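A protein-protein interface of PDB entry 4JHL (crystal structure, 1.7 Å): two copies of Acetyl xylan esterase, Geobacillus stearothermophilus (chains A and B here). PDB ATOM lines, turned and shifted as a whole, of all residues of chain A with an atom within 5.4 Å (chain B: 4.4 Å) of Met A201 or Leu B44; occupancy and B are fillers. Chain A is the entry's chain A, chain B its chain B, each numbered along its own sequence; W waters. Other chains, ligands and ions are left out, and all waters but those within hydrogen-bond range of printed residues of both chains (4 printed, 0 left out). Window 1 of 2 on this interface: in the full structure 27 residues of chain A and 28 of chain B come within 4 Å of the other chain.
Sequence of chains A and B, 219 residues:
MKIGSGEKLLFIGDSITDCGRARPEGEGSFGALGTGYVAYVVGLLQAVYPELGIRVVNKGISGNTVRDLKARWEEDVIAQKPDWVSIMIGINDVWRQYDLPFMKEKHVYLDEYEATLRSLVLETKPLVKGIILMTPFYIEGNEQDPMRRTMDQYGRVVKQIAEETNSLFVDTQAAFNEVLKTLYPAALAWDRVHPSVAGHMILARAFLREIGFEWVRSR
The side-chain hydroxyl (OG) of Ser A196 lies close to the backbone NH (N) of Ala A198 (3.3 Å).
O of Leu B208 lies within hydrogen-bond range of N of Phe B213, 3.0 Å away.
Among the printed residues, pairs that only touch across the chains: Trp A215 with Trp B215 (3.4 Å), Ala A198 with Gln B46 (3.6 Å), Ile A202 with Ala B47 (3.6 Å), Arg A205 with Val B48 (3.6 Å), Tyr A40 with Met B201 (3.7 Å), Trp A215 with Phe B213 (3.7 Å), Tyr A40 with Tyr B40 (3.7 Å), Met A201 with Tyr B40 (3.7 Å), Ala A198 with Gly B43 (3.7 Å), Met A201 with Met B201 (3.8 Å), Leu A44 with Met B201 (3.9 Å), Met A201 with Leu B44 (3.9 Å), Met A201 with Gly B43 (3.98 Å) and Trp A215 with Leu B208 (3.98 Å).
Water W2 bridges the side-chain amide nitrogen (NE2) of Gln B46 (2.5 Å) and the side-chain hydroxyl (OG) of Ser A196 (2.6 Å).
Water W1 lies within hydrogen-bond range of the backbone carbonyl oxygen (O) of Phe B213 (2.5 Å) and the indole nitrogen (NE1) of Trp A215 (2.9 Å).
Water W4 bridges O of Ala B47 (3.0 Å) and NH1 of Arg A205 (3.1 Å).
Water W3 bridges N of Ala A198 (3.3 Å) and OE1 of Gln B46 (3.4 Å).
Tyr B40 touches its own counterpart, Tyr A40.
Tyr A40 touches Met B201, and with the chains exchanged Met A201 touches Tyr B40.
Leu A44 touches Met B201, and with the chains exchanged Met A201 touches Leu B44.
Met A201 touches its own counterpart, Met B201.
Positions printed for both chains: 40, 44, 201 and 215.
Of the 15 pairs that touch across the chains among the printed residues, 7 have their exchanged pair printed and touching as well.
The guanidinium group of Arg A205 sits at hydrogen-bond distance from the backbone carbonyl oxygen of Trp B215, at 2.8 Å.
Of the printed residues of chain B, Met A201 touches Tyr B40, Gly B43, Leu B44 and Met B201.
Printed residues of chain B within 4 Å of Ile A202: Ala B47 (3.6 Å).
Printed residues of chain A within 4 Å of Ala B47: Ile A202.
Printed residues of chain B within 4 Å of Trp A215: Leu B208 (3.98 Å), Phe B213 (3.7 Å) and Trp B215 (3.4 Å).
Printed residues of chain A within 4 Å of Phe B213: Trp A215 (3.7 Å).
Leu B45 touches none of the printed residues of chain A.
The nearest residue of chain B that does not touch Met A201 is Ala B47 (4.3 Å).
Of the 14 printed residues of chain A, 7 touch a printed residue of chain B.
Along chain A the printed residues that touch a printed residue of chain B span positions 40 to 215.
Hydrophobic or aromatic side chains of chain B that line the printed part of chain A: Tyr B40, Leu B44, Ala B47, Val B48, Met B201, Leu B208, Phe B213 and Trp B215.
Among the printed residues, no Asp or Glu carboxylate lies within 4 Å of a Lys or Arg side-chain nitrogen of the other chain.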
ATOM      1  N   TYR A  40      33.778  26.649  -7.527  1.00  0.00           N
ATOM      2  CA  TYR A  40      33.733  25.241  -7.302  1.00  0.00           C
ATOM      3  C   TYR A  40      34.923  24.569  -8.005  1.00  0.00           C
ATOM      4  O   TYR A  40      35.570  23.675  -7.444  1.00  0.00           O
ATOM      5  CB  TYR A  40      32.445  24.634  -7.790  1.00  0.00           C
ATOM      6  CG  TYR A  40      31.181  25.066  -7.077  1.00  0.00           C
ATOM      7  CD1 TYR A  40      31.196  25.796  -5.899  1.00  0.00           C
ATOM      8  CD2 TYR A  40      29.991  24.715  -7.575  1.00  0.00           C
ATOM      9  CE1 TYR A  40      29.958  26.213  -5.301  1.00  0.00           C
ATOM     10  CE2 TYR A  40      28.804  25.072  -6.997  1.00  0.00           C
ATOM     11  CZ  TYR A  40      28.793  25.844  -5.885  1.00  0.00           C
ATOM     12  OH  TYR A  40      27.646  26.281  -5.251  1.00  0.00           O
ATOM     13  N   LEU A  44      37.845  22.480  -6.037  1.00  0.00           N
ATOM     14  CA  LEU A  44      38.189  21.135  -6.351  1.00  0.00           C
ATOM     15  C   LEU A  44      39.623  20.991  -6.773  1.00  0.00           C
ATOM     16  O   LEU A  44      40.297  19.984  -6.369  1.00  0.00           O
ATOM     17  CB  LEU A  44      37.268  20.577  -7.403  1.00  0.00           C
ATOM     18  CG  LEU A  44      35.910  20.109  -6.812  1.00  0.00           C
ATOM     19  CD1 LEU A  44      34.859  20.011  -7.899  1.00  0.00           C
ATOM     20  CD2 LEU A  44      36.051  18.798  -6.001  1.00  0.00           C
ATOM     21  N   SER A 196      20.618  26.165  -9.443  1.00  0.00           N
ATOM     22  CA  SER A 196      21.003  25.798  -8.055  1.00  0.00           C
ATOM     23  C   SER A 196      22.473  25.438  -7.977  1.00  0.00           C
ATOM     24  O   SER A 196      23.199  25.371  -8.993  1.00  0.00           O
ATOM     25  CB  SER A 196      20.291  24.564  -7.642  1.00  0.00           C
ATOM     26  OG  SER A 196      20.456  23.528  -8.524  1.00  0.00           O
ATOM     27  N   VAL A 197      22.957  25.100  -6.755  1.00  0.00           N
ATOM     28  CA  VAL A 197      24.268  24.609  -6.581  1.00  0.00           C
ATOM     29  C   VAL A 197      24.497  23.355  -7.492  1.00  0.00           C
ATOM     30  O   VAL A 197      25.555  23.220  -8.062  1.00  0.00           O
ATOM     31  CB  VAL A 197      24.458  24.173  -5.130  1.00  0.00           C
ATOM     32  CG1 VAL A 197      25.697  23.359  -4.902  1.00  0.00           C
ATOM     33  CG2 VAL A 197      24.434  25.440  -4.265  1.00  0.00           C
ATOM     34  N   ALA A 198      23.487  22.542  -7.622  1.00  0.00           N
ATOM     35  CA  ALA A 198      23.586  21.343  -8.477  1.00  0.00           C
ATOM     36  C   ALA A 198      23.923  21.753  -9.924  1.00  0.00           C
ATOM     37  O   ALA A 198      24.771  21.113 -10.561  1.00  0.00           O
ATOM     38  CB  ALA A 198      22.328  20.542  -8.415  1.00  0.00           C
ATOM     39  N   GLY A 199      23.278  22.782 -10.460  1.00  0.00           N
ATOM     40  CA  GLY A 199      23.662  23.267 -11.762  1.00  0.00           C
ATOM     41  C   GLY A 199      25.024  23.798 -11.937  1.00  0.00           C
ATOM     42  O   GLY A 199      25.711  23.558 -12.947  1.00  0.00           O
ATOM     43  N   HIS A 200      25.484  24.541 -10.939  1.00  0.00           N
ATOM     44  CA  HIS A 200      26.865  24.956 -10.951  1.00  0.00           C
ATOM     45  C   HIS A 200      27.841  23.813 -10.800  1.00  0.00           C
ATOM     46  O   HIS A 200      28.949  23.893 -11.328  1.00  0.00           O
ATOM     47  CB  HIS A 200      27.105  26.083  -9.919  1.00  0.00           C
ATOM     48  CG  HIS A 200      26.614  27.419 -10.364  1.00  0.00           C
ATOM     49  ND1 HIS A 200      27.333  28.204 -11.216  1.00  0.00           N
ATOM     50  CD2 HIS A 200      25.389  28.035 -10.255  1.00  0.00           C
ATOM     51  CE1 HIS A 200      26.656  29.275 -11.544  1.00  0.00           C
ATOM     52  NE2 HIS A 200      25.485  29.221 -10.948  1.00  0.00           N
ATOM     53  N   MET A 201      27.459  22.742 -10.113  1.00  0.00           N
ATOM     54  CA  MET A 201      28.267  21.531 -10.032  1.00  0.00           C
ATOM     55  C   MET A 201      28.307  20.800 -11.365  1.00  0.00           C
ATOM     56  O   MET A 201      29.352  20.351 -11.793  1.00  0.00           O
ATOM     57  CB  MET A 201      27.816  20.571  -8.887  1.00  0.00           C
ATOM     58  CG  MET A 201      28.167  21.051  -7.553  1.00  0.00           C
ATOM     59  SD  MET A 201      30.108  20.917  -7.276  1.00  0.00           S
ATOM     60  CE  MET A 201      29.546  21.420  -5.497  1.00  0.00           C
ATOM     61  N   ILE A 202      27.190  20.834 -12.096  1.00  0.00           N
ATOM     62  CA  ILE A 202      27.182  20.222 -13.451  1.00  0.00           C
ATOM     63  C   ILE A 202      28.169  20.974 -14.315  1.00  0.00           C
ATOM     64  O   ILE A 202      28.970  20.383 -15.047  1.00  0.00           O
ATOM     65  CB  ILE A 202      25.772  20.313 -14.006  1.00  0.00           C
ATOM     66  CG1 ILE A 202      24.823  19.335 -13.335  1.00  0.00           C
ATOM     67  CG2 ILE A 202      25.788  20.075 -15.528  1.00  0.00           C
ATOM     68  CD1 ILE A 202      23.333  19.497 -13.589  1.00  0.00           C
ATOM     69  N   LEU A 203      28.169  22.312 -14.240  1.00  0.00           N
ATOM     70  CA  LEU A 203      29.097  23.124 -15.002  1.00  0.00           C
ATOM     71  C   LEU A 203      30.554  22.876 -14.568  1.00  0.00           C
ATOM     72  O   LEU A 203      31.453  22.681 -15.394  1.00  0.00           O
ATOM     73  CB  LEU A 203      28.781  24.641 -14.883  1.00  0.00           C
ATOM     74  CG  LEU A 203      27.480  24.975 -15.562  1.00  0.00           C
ATOM     75  CD1 LEU A 203      27.110  26.331 -15.098  1.00  0.00           C
ATOM     76  CD2 LEU A 203      27.651  24.990 -17.093  1.00  0.00           C
ATOM     77  N   ALA A 204      30.834  22.925 -13.249  1.00  0.00           N
ATOM     78  CA  ALA A 204      32.187  22.750 -12.771  1.00  0.00           C
ATOM     79  C   ALA A 204      32.728  21.348 -13.216  1.00  0.00           C
ATOM     80  O   ALA A 204      33.892  21.234 -13.626  1.00  0.00           O
ATOM     81  CB  ALA A 204      32.209  22.800 -11.249  1.00  0.00           C
ATOM     82  N   ARG A 205      31.883  20.359 -13.110  1.00  0.00           N
ATOM     83  CA  ARG A 205      32.288  18.974 -13.438  1.00  0.00           C
ATOM     84  C   ARG A 205      32.607  18.871 -14.919  1.00  0.00           C
ATOM     85  O   ARG A 205      33.600  18.273 -15.323  1.00  0.00           O
ATOM     86  CB  ARG A 205      31.249  17.977 -13.035  1.00  0.00           C
ATOM     87  CG  ARG A 205      31.479  16.544 -13.468  1.00  0.00           C
ATOM     88  CD  ARG A 205      30.624  15.643 -12.629  1.00  0.00           C
ATOM     89  NE  ARG A 205      30.589  14.228 -13.027  1.00  0.00           N
ATOM     90  CZ  ARG A 205      29.732  13.746 -13.904  1.00  0.00           C
ATOM     91  NH1 ARG A 205      28.904  14.536 -14.566  1.00  0.00           N
ATOM     92  NH2 ARG A 205      29.738  12.460 -14.137  1.00  0.00           N
ATOM     93  N   ALA A 206      31.773  19.512 -15.714  1.00  0.00           N
ATOM     94  CA  ALA A 206      32.009  19.480 -17.224  1.00  0.00           C
ATOM     95  C   ALA A 206      33.320  20.153 -17.535  1.00  0.00           C
ATOM     96  O   ALA A 206      34.113  19.648 -18.380  1.00  0.00           O
ATOM     97  CB  ALA A 206      30.773  20.122 -17.930  1.00  0.00           C
ATOM     98  N   TRP A 215      39.148  12.767 -10.080  1.00  0.00           N
ATOM     99  CA  TRP A 215      38.547  12.854  -8.725  1.00  0.00           C
ATOM    100  C   TRP A 215      39.414  12.214  -7.653  1.00  0.00           C
ATOM    101  O   TRP A 215      39.638  12.756  -6.580  1.00  0.00           O
ATOM    102  CB  TRP A 215      37.188  12.221  -8.798  1.00  0.00           C
ATOM    103  CG  TRP A 215      36.427  12.086  -7.504  1.00  0.00           C
ATOM    104  CD1 TRP A 215      36.185  10.902  -6.837  1.00  0.00           C
ATOM    105  CD2 TRP A 215      35.733  13.095  -6.774  1.00  0.00           C
ATOM    106  NE1 TRP A 215      35.365  11.124  -5.737  1.00  0.00           N
ATOM    107  CE2 TRP A 215      35.113  12.458  -5.655  1.00  0.00           C
ATOM    108  CE3 TRP A 215      35.513  14.466  -6.973  1.00  0.00           C
ATOM    109  CZ2 TRP A 215      34.256  13.129  -4.792  1.00  0.00           C
ATOM    110  CZ3 TRP A 215      34.697  15.126  -6.075  1.00  0.00           C
ATOM    111  CH2 TRP A 215      34.095  14.447  -5.001  1.00  0.00           C
ATOM    112  N   TYR B  40      27.282  21.190  -1.071  1.00  0.00           N
ATOM    113  CA  TYR B  40      28.116  20.643  -2.151  1.00  0.00           C
ATOM    114  C   TYR B  40      27.828  19.169  -2.352  1.00  0.00           C
ATOM    115  O   TYR B  40      27.827  18.692  -3.503  1.00  0.00           O
ATOM    116  CB  TYR B  40      29.597  20.859  -1.840  1.00  0.00           C
ATOM    117  CG  TYR B  40      30.074  22.284  -1.756  1.00  0.00           C
ATOM    118  CD1 TYR B  40      29.282  23.369  -2.088  1.00  0.00           C
ATOM    119  CD2 TYR B  40      31.323  22.577  -1.262  1.00  0.00           C
ATOM    120  CE1 TYR B  40      29.738  24.668  -1.955  1.00  0.00           C
ATOM    121  CE2 TYR B  40      31.795  23.866  -1.204  1.00  0.00           C
ATOM    122  CZ  TYR B  40      30.981  24.911  -1.482  1.00  0.00           C
ATOM    123  OH  TYR B  40      31.423  26.210  -1.309  1.00  0.00           O
ATOM    124  N   VAL B  41      27.753  18.394  -1.248  1.00  0.00           N
ATOM    125  CA  VAL B  41      27.376  17.002  -1.339  1.00  0.00           C
ATOM    126  C   VAL B  41      26.058  16.831  -2.132  1.00  0.00           C
ATOM    127  O   VAL B  41      25.955  16.039  -3.108  1.00  0.00           O
ATOM    128  CB  VAL B  41      27.307  16.327   0.039  1.00  0.00           C
ATOM    129  CG1 VAL B  41      26.592  14.974  -0.070  1.00  0.00           C
ATOM    130  CG2 VAL B  41      28.689  16.221   0.677  1.00  0.00           C
ATOM    131  N   VAL B  42      25.036  17.605  -1.761  1.00  0.00           N
ATOM    132  CA  VAL B  42      23.763  17.523  -2.436  1.00  0.00           C
ATOM    133  C   VAL B  42      23.881  17.888  -3.925  1.00  0.00           C
ATOM    134  O   VAL B  42      23.291  17.236  -4.783  1.00  0.00           O
ATOM    135  CB  VAL B  42      22.714  18.311  -1.709  1.00  0.00           C
ATOM    136  CG1 VAL B  42      21.322  18.240  -2.359  1.00  0.00           C
ATOM    137  CG2 VAL B  42      22.543  17.853  -0.290  1.00  0.00           C
ATOM    138  N   GLY B  43      24.673  18.899  -4.236  1.00  0.00           N
ATOM    139  CA  GLY B  43      24.884  19.302  -5.589  1.00  0.00           C
ATOM    140  C   GLY B  43      25.493  18.234  -6.443  1.00  0.00           C
ATOM    141  O   GLY B  43      25.063  18.025  -7.562  1.00  0.00           O
ATOM    142  N   LEU B  44      26.528  17.607  -5.892  1.00  0.00           N
ATOM    143  CA  LEU B  44      27.211  16.543  -6.609  1.00  0.00           C
ATOM    144  C   LEU B  44      26.310  15.326  -6.747  1.00  0.00           C
ATOM    145  O   LEU B  44      26.350  14.701  -7.792  1.00  0.00           O
ATOM    146  CB  LEU B  44      28.506  16.188  -5.955  1.00  0.00           C
ATOM    147  CG  LEU B  44      29.601  17.199  -6.264  1.00  0.00           C
ATOM    148  CD1 LEU B  44      30.706  17.079  -5.260  1.00  0.00           C
ATOM    149  CD2 LEU B  44      30.013  17.056  -7.721  1.00  0.00           C
ATOM    150  N   LEU B  45      25.551  14.961  -5.716  1.00  0.00           N
ATOM    151  CA  LEU B  45      24.578  13.876  -5.817  1.00  0.00           C
ATOM    152  C   LEU B  45      23.498  14.117  -6.876  1.00  0.00           C
ATOM    153  O   LEU B  45      23.209  13.225  -7.681  1.00  0.00           O
ATOM    154  CB  LEU B  45      23.904  13.547  -4.494  1.00  0.00           C
ATOM    155  CG  LEU B  45      24.836  12.934  -3.443  1.00  0.00           C
ATOM    156  CD1 LEU B  45      24.184  12.811  -2.122  1.00  0.00           C
ATOM    157  CD2 LEU B  45      25.389  11.587  -3.876  1.00  0.00           C
ATOM    158  N   GLN B  46      22.995  15.326  -6.934  1.00  0.00           N
ATOM    159  CA  GLN B  46      22.005  15.667  -8.017  1.00  0.00           C
ATOM    160  C   GLN B  46      22.676  15.750  -9.389  1.00  0.00           C
ATOM    161  O   GLN B  46      22.065  15.337 -10.393  1.00  0.00           O
ATOM    162  CB  GLN B  46      21.353  16.948  -7.590  1.00  0.00           C
ATOM    163  CG  GLN B  46      19.995  17.198  -8.170  1.00  0.00           C
ATOM    164  CD  GLN B  46      19.435  18.563  -7.638  1.00  0.00           C
ATOM    165  OE1 GLN B  46      19.707  19.073  -6.465  1.00  0.00           O
ATOM    166  NE2 GLN B  46      18.732  19.171  -8.483  1.00  0.00           N
ATOM    167  N   ALA B  47      23.922  16.226  -9.503  1.00  0.00           N
ATOM    168  CA  ALA B  47      24.600  16.344 -10.787  1.00  0.00           C
ATOM    169  C   ALA B  47      24.938  14.962 -11.397  1.00  0.00           C
ATOM    170  O   ALA B  47      24.846  14.754 -12.622  1.00  0.00           O
ATOM    171  CB  ALA B  47      25.845  17.128 -10.643  1.00  0.00           C
ATOM    172  N   VAL B  48      25.278  14.008 -10.517  1.00  0.00           N
ATOM    173  CA  VAL B  48      25.762  12.678 -10.949  1.00  0.00           C
ATOM    174  C   VAL B  48      24.695  11.572 -10.753  1.00  0.00           C
ATOM    175  O   VAL B  48      24.690  10.592 -11.554  1.00  0.00           O
ATOM    176  CB  VAL B  48      27.109  12.369 -10.286  1.00  0.00           C
ATOM    177  CG1 VAL B  48      27.717  11.079 -10.850  1.00  0.00           C
ATOM    178  CG2 VAL B  48      28.102  13.517 -10.457  1.00  0.00           C
ATOM    179  N   MET B 201      35.137  21.674   0.016  1.00  0.00           N
ATOM    180  CA  MET B 201      35.220  20.687  -1.015  1.00  0.00           C
ATOM    181  C   MET B 201      36.029  19.513  -0.515  1.00  0.00           C
ATOM    182  O   MET B 201      35.708  18.357  -0.829  1.00  0.00           O
ATOM    183  CB  MET B 201      35.839  21.178  -2.382  1.00  0.00           C
ATOM    184  CG  MET B 201      34.927  22.035  -3.127  1.00  0.00           C
ATOM    185  SD  MET B 201      33.502  20.927  -3.904  1.00  0.00           S
ATOM    186  CE  MET B 201      33.058  22.627  -4.803  1.00  0.00           C
ATOM    187  N   LEU B 208      31.702  11.986   0.314  1.00  0.00           N
ATOM    188  CA  LEU B 208      31.271  11.220  -0.875  1.00  0.00           C
ATOM    189  C   LEU B 208      32.095   9.955  -1.125  1.00  0.00           C
ATOM    190  O   LEU B 208      31.550   8.895  -1.497  1.00  0.00           O
ATOM    191  CB  LEU B 208      31.346  12.123  -2.061  1.00  0.00           C
ATOM    192  CG  LEU B 208      30.245  13.224  -2.107  1.00  0.00           C
ATOM    193  CD1 LEU B 208      30.588  14.279  -3.122  1.00  0.00           C
ATOM    194  CD2 LEU B 208      28.858  12.696  -2.329  1.00  0.00           C
ATOM    195  N   PHE B 213      30.266   7.263  -3.682  1.00  0.00           N
ATOM    196  CA  PHE B 213      30.078   8.081  -4.894  1.00  0.00           C
ATOM    197  C   PHE B 213      31.159   7.849  -5.950  1.00  0.00           C
ATOM    198  O   PHE B 213      32.376   7.718  -5.681  1.00  0.00           O
ATOM    199  CB  PHE B 213      30.315   9.538  -4.451  1.00  0.00           C
ATOM    200  CG  PHE B 213      30.241  10.595  -5.529  1.00  0.00           C
ATOM    201  CD1 PHE B 213      29.023  11.172  -5.859  1.00  0.00           C
ATOM    202  CD2 PHE B 213      31.389  11.140  -6.017  1.00  0.00           C
ATOM    203  CE1 PHE B 213      28.989  12.187  -6.811  1.00  0.00           C
ATOM    204  CE2 PHE B 213      31.400  12.219  -6.914  1.00  0.00           C
ATOM    205  CZ  PHE B 213      30.188  12.722  -7.306  1.00  0.00           C
ATOM    206  N   TRP B 215      32.605   9.752  -9.457  1.00  0.00           N
ATOM    207  CA  TRP B 215      32.638  10.988 -10.176  1.00  0.00           C
ATOM    208  C   TRP B 215      32.132  10.832 -11.568  1.00  0.00           C
ATOM    209  O   TRP B 215      31.413  11.687 -12.076  1.00  0.00           O
ATOM    210  CB  TRP B 215      34.047  11.488 -10.178  1.00  0.00           C
ATOM    211  CG  TRP B 215      34.396  12.701 -10.979  1.00  0.00           C
ATOM    212  CD1 TRP B 215      35.145  12.757 -12.125  1.00  0.00           C
ATOM    213  CD2 TRP B 215      34.112  14.090 -10.658  1.00  0.00           C
ATOM    214  NE1 TRP B 215      35.321  14.032 -12.521  1.00  0.00           N
ATOM    215  CE2 TRP B 215      34.728  14.873 -11.696  1.00  0.00           C
ATOM    216  CE3 TRP B 215      33.441  14.734  -9.648  1.00  0.00           C
ATOM    217  CZ2 TRP B 215      34.655  16.231 -11.714  1.00  0.00           C
ATOM    218  CZ3 TRP B 215      33.372  16.114  -9.681  1.00  0.00           C
ATOM    219  CH2 TRP B 215      33.977  16.839 -10.685  1.00  0.00           C
HETATM  220  O   HOH W   1      34.509   8.626  -4.655  1.00  0.00           O
HETATM  221  O   HOH W   2      18.674  21.615  -8.103  1.00  0.00           O
HETATM  222  O   HOH W   3      21.233  21.905  -5.263  1.00  0.00           O
HETATM  223  O   HOH W   4      26.367  16.296 -14.761  1.00  0.00           O
